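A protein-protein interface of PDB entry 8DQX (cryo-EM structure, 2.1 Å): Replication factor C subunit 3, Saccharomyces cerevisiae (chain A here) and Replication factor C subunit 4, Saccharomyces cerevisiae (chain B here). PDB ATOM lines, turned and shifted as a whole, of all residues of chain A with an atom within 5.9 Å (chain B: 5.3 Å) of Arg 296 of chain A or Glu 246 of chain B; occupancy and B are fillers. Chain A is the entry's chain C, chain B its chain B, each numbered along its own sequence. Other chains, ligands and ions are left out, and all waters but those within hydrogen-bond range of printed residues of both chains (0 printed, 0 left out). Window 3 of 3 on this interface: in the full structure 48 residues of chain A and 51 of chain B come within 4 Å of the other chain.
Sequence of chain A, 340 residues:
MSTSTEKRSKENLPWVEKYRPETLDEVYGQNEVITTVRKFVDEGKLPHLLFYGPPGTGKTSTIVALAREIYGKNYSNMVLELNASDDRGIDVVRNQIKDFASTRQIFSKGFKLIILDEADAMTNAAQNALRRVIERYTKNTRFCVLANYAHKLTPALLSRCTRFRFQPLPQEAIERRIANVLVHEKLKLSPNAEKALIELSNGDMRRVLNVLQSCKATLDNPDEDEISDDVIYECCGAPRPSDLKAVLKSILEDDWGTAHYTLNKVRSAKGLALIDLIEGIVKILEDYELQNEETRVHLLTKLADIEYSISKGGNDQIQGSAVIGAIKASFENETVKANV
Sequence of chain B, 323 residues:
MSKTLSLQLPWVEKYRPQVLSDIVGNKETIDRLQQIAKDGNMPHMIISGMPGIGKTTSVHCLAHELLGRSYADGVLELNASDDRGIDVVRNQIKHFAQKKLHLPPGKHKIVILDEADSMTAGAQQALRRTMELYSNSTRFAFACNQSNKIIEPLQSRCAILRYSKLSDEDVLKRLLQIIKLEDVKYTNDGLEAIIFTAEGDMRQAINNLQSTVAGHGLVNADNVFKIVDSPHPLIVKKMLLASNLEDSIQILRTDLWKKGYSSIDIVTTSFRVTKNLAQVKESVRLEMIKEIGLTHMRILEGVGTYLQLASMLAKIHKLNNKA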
ATOM      1  N   LEU A 285       4.329  -4.401  -9.486  1.00  0.00           N
ATOM      2  CA  LEU A 285       4.373  -3.309  -8.519  1.00  0.00           C
ATOM      3  C   LEU A 285       2.995  -2.717  -8.266  1.00  0.00           C
ATOM      4  O   LEU A 285       2.756  -2.148  -7.195  1.00  0.00           O
ATOM      5  CB  LEU A 285       5.329  -2.216  -9.003  1.00  0.00           C
ATOM      6  CG  LEU A 285       6.820  -2.456  -8.745  1.00  0.00           C
ATOM      7  CD1 LEU A 285       7.675  -1.447  -9.481  1.00  0.00           C
ATOM      8  CD2 LEU A 285       7.113  -2.416  -7.259  1.00  0.00           C
ATOM      9  N   GLU A 286       2.079  -2.835  -9.229  1.00  0.00           N
ATOM     10  CA  GLU A 286       0.730  -2.321  -9.014  1.00  0.00           C
ATOM     11  C   GLU A 286       0.083  -2.935  -7.779  1.00  0.00           C
ATOM     12  O   GLU A 286      -0.695  -2.264  -7.091  1.00  0.00           O
ATOM     13  CB  GLU A 286      -0.133  -2.576 -10.249  1.00  0.00           C
ATOM     14  CG  GLU A 286       0.331  -1.822 -11.483  1.00  0.00           C
ATOM     15  CD  GLU A 286      -0.490  -0.574 -11.745  1.00  0.00           C
ATOM     16  OE1 GLU A 286      -1.629  -0.710 -12.239  1.00  0.00           O
ATOM     17  OE2 GLU A 286       0.000   0.538 -11.455  1.00  0.00           O
ATOM     18  N   ASP A 287       0.402  -4.191  -7.466  1.00  0.00           N
ATOM     19  CA  ASP A 287      -0.195  -4.863  -6.317  1.00  0.00           C
ATOM     20  C   ASP A 287       0.509  -4.553  -5.004  1.00  0.00           C
ATOM     21  O   ASP A 287       0.034  -4.990  -3.950  1.00  0.00           O
ATOM     22  CB  ASP A 287      -0.197  -6.375  -6.538  1.00  0.00           C
ATOM     23  CG  ASP A 287      -1.175  -6.804  -7.612  1.00  0.00           C
ATOM     24  OD1 ASP A 287      -1.993  -5.964  -8.039  1.00  0.00           O
ATOM     25  OD2 ASP A 287      -1.125  -7.982  -8.026  1.00  0.00           O
ATOM     26  N   TYR A 288       1.620  -3.825  -5.029  1.00  0.00           N
ATOM     27  CA  TYR A 288       2.314  -3.497  -3.794  1.00  0.00           C
ATOM     28  C   TYR A 288       1.479  -2.529  -2.965  1.00  0.00           C
ATOM     29  O   TYR A 288       0.829  -1.628  -3.501  1.00  0.00           O
ATOM     30  CB  TYR A 288       3.679  -2.875  -4.091  1.00  0.00           C
ATOM     31  CG  TYR A 288       4.824  -3.865  -4.172  1.00  0.00           C
ATOM     32  CD1 TYR A 288       4.697  -5.046  -4.886  1.00  0.00           C
ATOM     33  CD2 TYR A 288       6.037  -3.607  -3.546  1.00  0.00           C
ATOM     34  CE1 TYR A 288       5.741  -5.949  -4.974  1.00  0.00           C
ATOM     35  CE2 TYR A 288       7.089  -4.506  -3.623  1.00  0.00           C
ATOM     36  CZ  TYR A 288       6.933  -5.674  -4.342  1.00  0.00           C
ATOM     37  OH  TYR A 288       7.969  -6.575  -4.425  1.00  0.00           O
ATOM     38  N   GLU A 289       1.494  -2.727  -1.653  1.00  0.00           N
ATOM     39  CA  GLU A 289       0.957  -1.753  -0.714  1.00  0.00           C
ATOM     40  C   GLU A 289       2.088  -0.823  -0.297  1.00  0.00           C
ATOM     41  O   GLU A 289       3.102  -1.277   0.241  1.00  0.00           O
ATOM     42  CB  GLU A 289       0.348  -2.449   0.502  1.00  0.00           C
ATOM     43  CG  GLU A 289      -1.063  -2.968   0.274  1.00  0.00           C
ATOM     44  CD  GLU A 289      -2.080  -1.853   0.149  1.00  0.00           C
ATOM     45  OE1 GLU A 289      -1.819  -0.746   0.666  1.00  0.00           O
ATOM     46  OE2 GLU A 289      -3.141  -2.081  -0.470  1.00  0.00           O
ATOM     47  N   LEU A 290       1.924   0.470  -0.558  1.00  0.00           N
ATOM     48  CA  LEU A 290       2.965   1.457  -0.321  1.00  0.00           C
ATOM     49  C   LEU A 290       2.506   2.461   0.725  1.00  0.00           C
ATOM     50  O   LEU A 290       1.375   2.952   0.677  1.00  0.00           O
ATOM     51  CB  LEU A 290       3.336   2.191  -1.609  1.00  0.00           C
ATOM     52  CG  LEU A 290       3.773   1.338  -2.799  1.00  0.00           C
ATOM     53  CD1 LEU A 290       3.739   2.168  -4.065  1.00  0.00           C
ATOM     54  CD2 LEU A 290       5.157   0.751  -2.575  1.00  0.00           C
ATOM     55  N   ASN A 292       3.792   5.516   1.164  1.00  0.00           N
ATOM     56  CA  ASN A 292       3.855   6.875   0.647  1.00  0.00           C
ATOM     57  C   ASN A 292       3.316   6.921  -0.776  1.00  0.00           C
ATOM     58  O   ASN A 292       3.745   6.146  -1.638  1.00  0.00           O
ATOM     59  CB  ASN A 292       5.292   7.395   0.688  1.00  0.00           C
ATOM     60  CG  ASN A 292       5.393   8.869   0.353  1.00  0.00           C
ATOM     61  OD1 ASN A 292       4.439   9.479  -0.128  1.00  0.00           O
ATOM     62  ND2 ASN A 292       6.559   9.451   0.605  1.00  0.00           N
ATOM     63  N   GLU A 293       2.378   7.837  -1.016  1.00  0.00           N
ATOM     64  CA  GLU A 293       1.891   8.070  -2.369  1.00  0.00           C
ATOM     65  C   GLU A 293       2.998   8.591  -3.277  1.00  0.00           C
ATOM     66  O   GLU A 293       2.955   8.386  -4.500  1.00  0.00           O
ATOM     67  CB  GLU A 293       0.725   9.053  -2.320  1.00  0.00           C
ATOM     68  CG  GLU A 293       0.092   9.352  -3.655  1.00  0.00           C
ATOM     69  CD  GLU A 293      -0.938  10.446  -3.543  1.00  0.00           C
ATOM     70  OE1 GLU A 293      -0.534  11.606  -3.324  1.00  0.00           O
ATOM     71  OE2 GLU A 293      -2.146  10.155  -3.673  1.00  0.00           O
ATOM     72  N   GLU A 294       4.001   9.255  -2.701  1.00  0.00           N
ATOM     73  CA  GLU A 294       5.093   9.779  -3.511  1.00  0.00           C
ATOM     74  C   GLU A 294       5.872   8.657  -4.190  1.00  0.00           C
ATOM     75  O   GLU A 294       6.379   8.837  -5.302  1.00  0.00           O
ATOM     76  CB  GLU A 294       6.024  10.628  -2.638  1.00  0.00           C
ATOM     77  CG  GLU A 294       6.875  11.658  -3.391  1.00  0.00           C
ATOM     78  CD  GLU A 294       6.260  12.110  -4.709  1.00  0.00           C
ATOM     79  OE1 GLU A 294       5.154  12.689  -4.678  1.00  0.00           O
ATOM     80  OE2 GLU A 294       6.867  11.871  -5.773  1.00  0.00           O
ATOM     81  N   THR A 295       5.976   7.495  -3.538  1.00  0.00           N
ATOM     82  CA  THR A 295       6.616   6.344  -4.168  1.00  0.00           C
ATOM     83  C   THR A 295       5.892   5.961  -5.453  1.00  0.00           C
ATOM     84  O   THR A 295       6.517   5.787  -6.506  1.00  0.00           O
ATOM     85  CB  THR A 295       6.639   5.163  -3.193  1.00  0.00           C
ATOM     86  OG1 THR A 295       7.267   5.565  -1.969  1.00  0.00           O
ATOM     87  CG2 THR A 295       7.399   3.985  -3.780  1.00  0.00           C
ATOM     88  N   ARG A 296       4.565   5.835  -5.381  1.00  0.00           N
ATOM     89  CA  ARG A 296       3.782   5.510  -6.567  1.00  0.00           C
ATOM     90  C   ARG A 296       3.951   6.577  -7.640  1.00  0.00           C
ATOM     91  O   ARG A 296       4.108   6.258  -8.825  1.00  0.00           O
ATOM     92  CB  ARG A 296       2.308   5.347  -6.188  1.00  0.00           C
ATOM     93  CG  ARG A 296       1.406   4.880  -7.326  1.00  0.00           C
ATOM     94  CD  ARG A 296       1.506   3.386  -7.586  1.00  0.00           C
ATOM     95  NE  ARG A 296       1.084   2.585  -6.443  1.00  0.00           N
ATOM     96  CZ  ARG A 296       1.331   1.290  -6.301  1.00  0.00           C
ATOM     97  NH1 ARG A 296       1.992   0.606  -7.222  1.00  0.00           N
ATOM     98  NH2 ARG A 296       0.909   0.665  -5.206  1.00  0.00           N
ATOM     99  N   VAL A 297       3.932   7.852  -7.240  1.00  0.00           N
ATOM    100  CA  VAL A 297       4.046   8.938  -8.212  1.00  0.00           C
ATOM    101  C   VAL A 297       5.373   8.852  -8.959  1.00  0.00           C
ATOM    102  O   VAL A 297       5.417   8.881 -10.199  1.00  0.00           O
ATOM    103  CB  VAL A 297       3.884  10.298  -7.510  1.00  0.00           C
ATOM    104  CG1 VAL A 297       4.332  11.436  -8.418  1.00  0.00           C
ATOM    105  CG2 VAL A 297       2.445  10.498  -7.070  1.00  0.00           C
ATOM    106  N   HIS A 298       6.476   8.750  -8.213  1.00  0.00           N
ATOM    107  CA  HIS A 298       7.788   8.683  -8.846  1.00  0.00           C
ATOM    108  C   HIS A 298       7.896   7.460  -9.747  1.00  0.00           C
ATOM    109  O   HIS A 298       8.350   7.561 -10.895  1.00  0.00           O
ATOM    110  CB  HIS A 298       8.894   8.668  -7.791  1.00  0.00           C
ATOM    111  CG  HIS A 298       9.152  10.003  -7.160  1.00  0.00           C
ATOM    112  ND1 HIS A 298       9.427  10.149  -5.818  1.00  0.00           N
ATOM    113  CD2 HIS A 298       9.176  11.250  -7.686  1.00  0.00           C
ATOM    114  CE1 HIS A 298       9.621  11.427  -5.546  1.00  0.00           C
ATOM    115  NE2 HIS A 298       9.469  12.117  -6.662  1.00  0.00           N
ATOM    116  N   LEU A 299       7.479   6.293  -9.247  1.00  0.00           N
ATOM    117  CA  LEU A 299       7.567   5.084 -10.056  1.00  0.00           C
ATOM    118  C   LEU A 299       6.846   5.274 -11.382  1.00  0.00           C
ATOM    119  O   LEU A 299       7.427   5.065 -12.453  1.00  0.00           O
ATOM    120  CB  LEU A 299       6.980   3.891  -9.302  1.00  0.00           C
ATOM    121  CG  LEU A 299       7.908   3.102  -8.373  1.00  0.00           C
ATOM    122  CD1 LEU A 299       7.089   2.273  -7.407  1.00  0.00           C
ATOM    123  CD2 LEU A 299       8.864   2.221  -9.165  1.00  0.00           C
ATOM    124  N   LEU A 300       5.581   5.701 -11.327  1.00  0.00           N
ATOM    125  CA  LEU A 300       4.778   5.766 -12.542  1.00  0.00           C
ATOM    126  C   LEU A 300       5.352   6.779 -13.524  1.00  0.00           C
ATOM    127  O   LEU A 300       5.517   6.477 -14.712  1.00  0.00           O
ATOM    128  CB  LEU A 300       3.322   6.098 -12.191  1.00  0.00           C
ATOM    129  CG  LEU A 300       2.535   4.980 -11.496  1.00  0.00           C
ATOM    130  CD1 LEU A 300       1.164   5.470 -11.051  1.00  0.00           C
ATOM    131  CD2 LEU A 300       2.393   3.749 -12.392  1.00  0.00           C
ATOM    132  N   THR A 301       5.691   7.981 -13.046  1.00  0.00           N
ATOM    133  CA  THR A 301       6.165   9.009 -13.969  1.00  0.00           C
ATOM    134  C   THR A 301       7.492   8.606 -14.614  1.00  0.00           C
ATOM    135  O   THR A 301       7.649   8.698 -15.840  1.00  0.00           O
ATOM    136  CB  THR A 301       6.284  10.358 -13.251  1.00  0.00           C
ATOM    137  OG1 THR A 301       7.094  10.227 -12.078  1.00  0.00           O
ATOM    138  CG2 THR A 301       4.903  10.880 -12.859  1.00  0.00           C
ATOM    139  N   ASN B 244      -7.324  10.782  -3.532  1.00  0.00           N
ATOM    140  CA  ASN B 244      -6.019  10.138  -3.465  1.00  0.00           C
ATOM    141  C   ASN B 244      -5.736   9.400  -4.765  1.00  0.00           C
ATOM    142  O   ASN B 244      -6.654   9.014  -5.493  1.00  0.00           O
ATOM    143  CB  ASN B 244      -5.928   9.172  -2.281  1.00  0.00           C
ATOM    144  CG  ASN B 244      -7.014   8.137  -2.296  1.00  0.00           C
ATOM    145  OD1 ASN B 244      -6.778   6.981  -2.633  1.00  0.00           O
ATOM    146  ND2 ASN B 244      -8.223   8.543  -1.926  1.00  0.00           N
ATOM    147  N   LEU B 245      -4.446   9.211  -5.050  1.00  0.00           N
ATOM    148  CA  LEU B 245      -4.048   8.652  -6.336  1.00  0.00           C
ATOM    149  C   LEU B 245      -4.570   7.230  -6.512  1.00  0.00           C
ATOM    150  O   LEU B 245      -4.967   6.844  -7.616  1.00  0.00           O
ATOM    151  CB  LEU B 245      -2.522   8.693  -6.475  1.00  0.00           C
ATOM    152  CG  LEU B 245      -1.940   8.074  -7.749  1.00  0.00           C
ATOM    153  CD1 LEU B 245      -2.548   8.698  -9.003  1.00  0.00           C
ATOM    154  CD2 LEU B 245      -0.422   8.203  -7.772  1.00  0.00           C
ATOM    155  N   GLU B 246      -4.585   6.438  -5.438  1.00  0.00           N
ATOM    156  CA  GLU B 246      -4.961   5.034  -5.572  1.00  0.00           C
ATOM    157  C   GLU B 246      -6.413   4.874  -6.014  1.00  0.00           C
ATOM    158  O   GLU B 246      -6.715   4.015  -6.846  1.00  0.00           O
ATOM    159  CB  GLU B 246      -4.711   4.289  -4.261  1.00  0.00           C
ATOM    160  CG  GLU B 246      -3.237   4.157  -3.886  1.00  0.00           C
ATOM    161  CD  GLU B 246      -2.345   3.766  -5.060  1.00  0.00           C
ATOM    162  OE1 GLU B 246      -2.621   2.735  -5.707  1.00  0.00           O
ATOM    163  OE2 GLU B 246      -1.369   4.494  -5.334  1.00  0.00           O
ATOM    164  N   ASP B 247      -7.328   5.689  -5.483  1.00  0.00           N
ATOM    165  CA  ASP B 247      -8.724   5.581  -5.904  1.00  0.00           C
ATOM    166  C   ASP B 247      -8.916   6.027  -7.351  1.00  0.00           C
ATOM    167  O   ASP B 247      -9.708   5.430  -8.092  1.00  0.00           O
ATOM    168  CB  ASP B 247      -9.626   6.394  -4.979  1.00  0.00           C
ATOM    169  CG  ASP B 247      -9.362   6.117  -3.519  1.00  0.00           C
ATOM    170  OD1 ASP B 247      -8.689   5.108  -3.215  1.00  0.00           O
ATOM    171  OD2 ASP B 247      -9.828   6.904  -2.672  1.00  0.00           O
ATOM    172  N   SER B 248      -8.220   7.087  -7.767  1.00  0.00           N
ATOM    173  CA  SER B 248      -8.308   7.513  -9.160  1.00  0.00           C
ATOM    174  C   SER B 248      -7.777   6.430 -10.093  1.00  0.00           C
ATOM    175  O   SER B 248      -8.379   6.141 -11.135  1.00  0.00           O
ATOM    176  CB  SER B 248      -7.547   8.826  -9.357  1.00  0.00           C
ATOM    177  OG  SER B 248      -6.150   8.622  -9.387  1.00  0.00           O
ATOM    178  N   ILE B 249      -6.658   5.806  -9.722  1.00  0.00           N
ATOM    179  CA  ILE B 249      -6.117   4.717 -10.527  1.00  0.00           C
ATOM    180  C   ILE B 249      -7.075   3.532 -10.527  1.00  0.00           C
ATOM    181  O   ILE B 249      -7.225   2.844 -11.540  1.00  0.00           O
ATOM    182  CB  ILE B 249      -4.716   4.325 -10.021  1.00  0.00           C
ATOM    183  CG1 ILE B 249      -3.654   5.226 -10.657  1.00  0.00           C
ATOM    184  CG2 ILE B 249      -4.416   2.863 -10.330  1.00  0.00           C
ATOM    185  CD1 ILE B 249      -2.314   5.181  -9.957  1.00  0.00           C
ATOM    186  N   GLN B 250      -7.733   3.273  -9.398  1.00  0.00           N
ATOM    187  CA  GLN B 250      -8.698   2.180  -9.332  1.00  0.00           C
ATOM    188  C   GLN B 250      -9.863   2.418 -10.283  1.00  0.00           C
ATOM    189  O   GLN B 250     -10.311   1.494 -10.973  1.00  0.00           O
ATOM    190  CB  GLN B 250      -9.192   2.018  -7.893  1.00  0.00           C
ATOM    191  CG  GLN B 250     -10.453   1.183  -7.727  1.00  0.00           C
ATOM    192  CD  GLN B 250     -10.407  -0.133  -8.471  1.00  0.00           C
ATOM    193  OE1 GLN B 250     -11.434  -0.621  -8.943  1.00  0.00           O
ATOM    194  NE2 GLN B 250      -9.219  -0.726  -8.570  1.00  0.00           N
ATOM    195  N   ILE B 251     -10.366   3.655 -10.334  1.00  0.00           N
ATOM    196  CA  ILE B 251     -11.433   3.981 -11.279  1.00  0.00           C
ATOM    197  C   ILE B 251     -10.943   3.792 -12.710  1.00  0.00           C
ATOM    198  O   ILE B 251     -11.614   3.163 -13.536  1.00  0.00           O
ATOM    199  CB  ILE B 251     -11.948   5.413 -11.046  1.00  0.00           C
ATOM    200  CG1 ILE B 251     -12.669   5.513  -9.699  1.00  0.00           C
ATOM    201  CG2 ILE B 251     -12.885   5.829 -12.165  1.00  0.00           C
ATOM    202  CD1 ILE B 251     -12.656   6.895  -9.107  1.00  0.00           C
ATOM    203  N   ALA B 314      -0.992  10.382 -12.052  1.00  0.00           N
ATOM    204  CA  ALA B 314      -0.025  10.731 -11.016  1.00  0.00           C
ATOM    205  C   ALA B 314       0.388  12.194 -11.114  1.00  0.00           C
ATOM    206  O   ALA B 314       0.505  12.886 -10.097  1.00  0.00           O
ATOM    207  CB  ALA B 314       1.199   9.824 -11.116  1.00  0.00           C
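Of the 16 printed residues of chain A, 4 touch a printed residue of chain B.
Hydrophobic or aromatic side chains of chain A that line the printed part of chain B: Val 297 and Leu 300.
Printed residues of chain B that touch a printed residue of chain A: Asn 244, Leu 245, Glu 246 and Ile 249.
Along chain B the printed residues that touch a printed residue of chain A span positions 244 to 249.
Among the printed residues, 6 pairs touch across the chains.
Among the printed residues, Asp or Glu carboxylates within 4 Å of a Lys or Arg side-chain nitrogen of the other chain: Arg 296 of chain A with Glu 246 of chain B (3.3 Å).
The backbone carbonyl oxygen of Tyr 288 of chain A lies within hydrogen-bond range of the guanidinium group of Arg 296 of chain A (2.9 Å).
O of Leu 245 of chain B lies within hydrogen-bond range of OG of Ser 248 of chain B, 2.8 Å away.
The side-chain hydroxyl (OG1) of Thr 301 of chain A lies within hydrogen-bond range of the backbone carbonyl oxygen (O) of Val 297 of chain A.
ND2 of Asn 244 of chain B sits at hydrogen-bond distance from OD2 of Asp 247 of chain B.
O of Leu 285 of chain A is in hydrogen-bond range of NH1 of Arg 296 of chain A (2.9 Å).
OE2 of Glu 246 of chain B lies within salt-bridge range of NE of Arg 296 of chain A, 3.3 Å away.
The side-chain carboxylate (OE2) of Glu 293 of chain A sits at hydrogen-bond distance from the backbone NH (N) of Leu 245 of chain B (2.8 Å).
Leu 285 of chain A touches none of the printed residues of chain B.
Asp 287 of chain A touches none of the printed residues of chain B.
Of the printed residues of chain B, Glu 293 of chain A touches Asn 244 (3.8 Å) and Leu 245 (2.8 Å).
Of chain B, only Leu 245 and Glu 246 come within 4 Å of Arg 296 of chain A.
Printed residues of chain B within 4 Å of Leu 300 of chain A: Ile 249.
Glu 246 of chain B touches just one residue of chain A: Arg 296.
Of the printed residues of chain A, Ile 249 of chain B touches Leu 300 (3.7 Å).
The nearest residue of chain B that does not touch Arg 296 of chain A is Ile 249 of chain B (4.6 Å).
The nearest residue of chain A that does not touch Glu 246 of chain B is Glu 293 of chain A (4.8 Å).
The nearest printed residue of chain A that does not touch Ile 249 of chain B is Arg 296 of chain A (4.6 Å).
Among the printed residues, merely in contact across the chains: Glu 293 of chain A with Asn 244 of chain B, Arg 296 of chain A with Leu 245 of chain B, Val 297 of chain A with Leu 245 of chain B and Leu 300 of chain A with Ile 249 of chain B.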
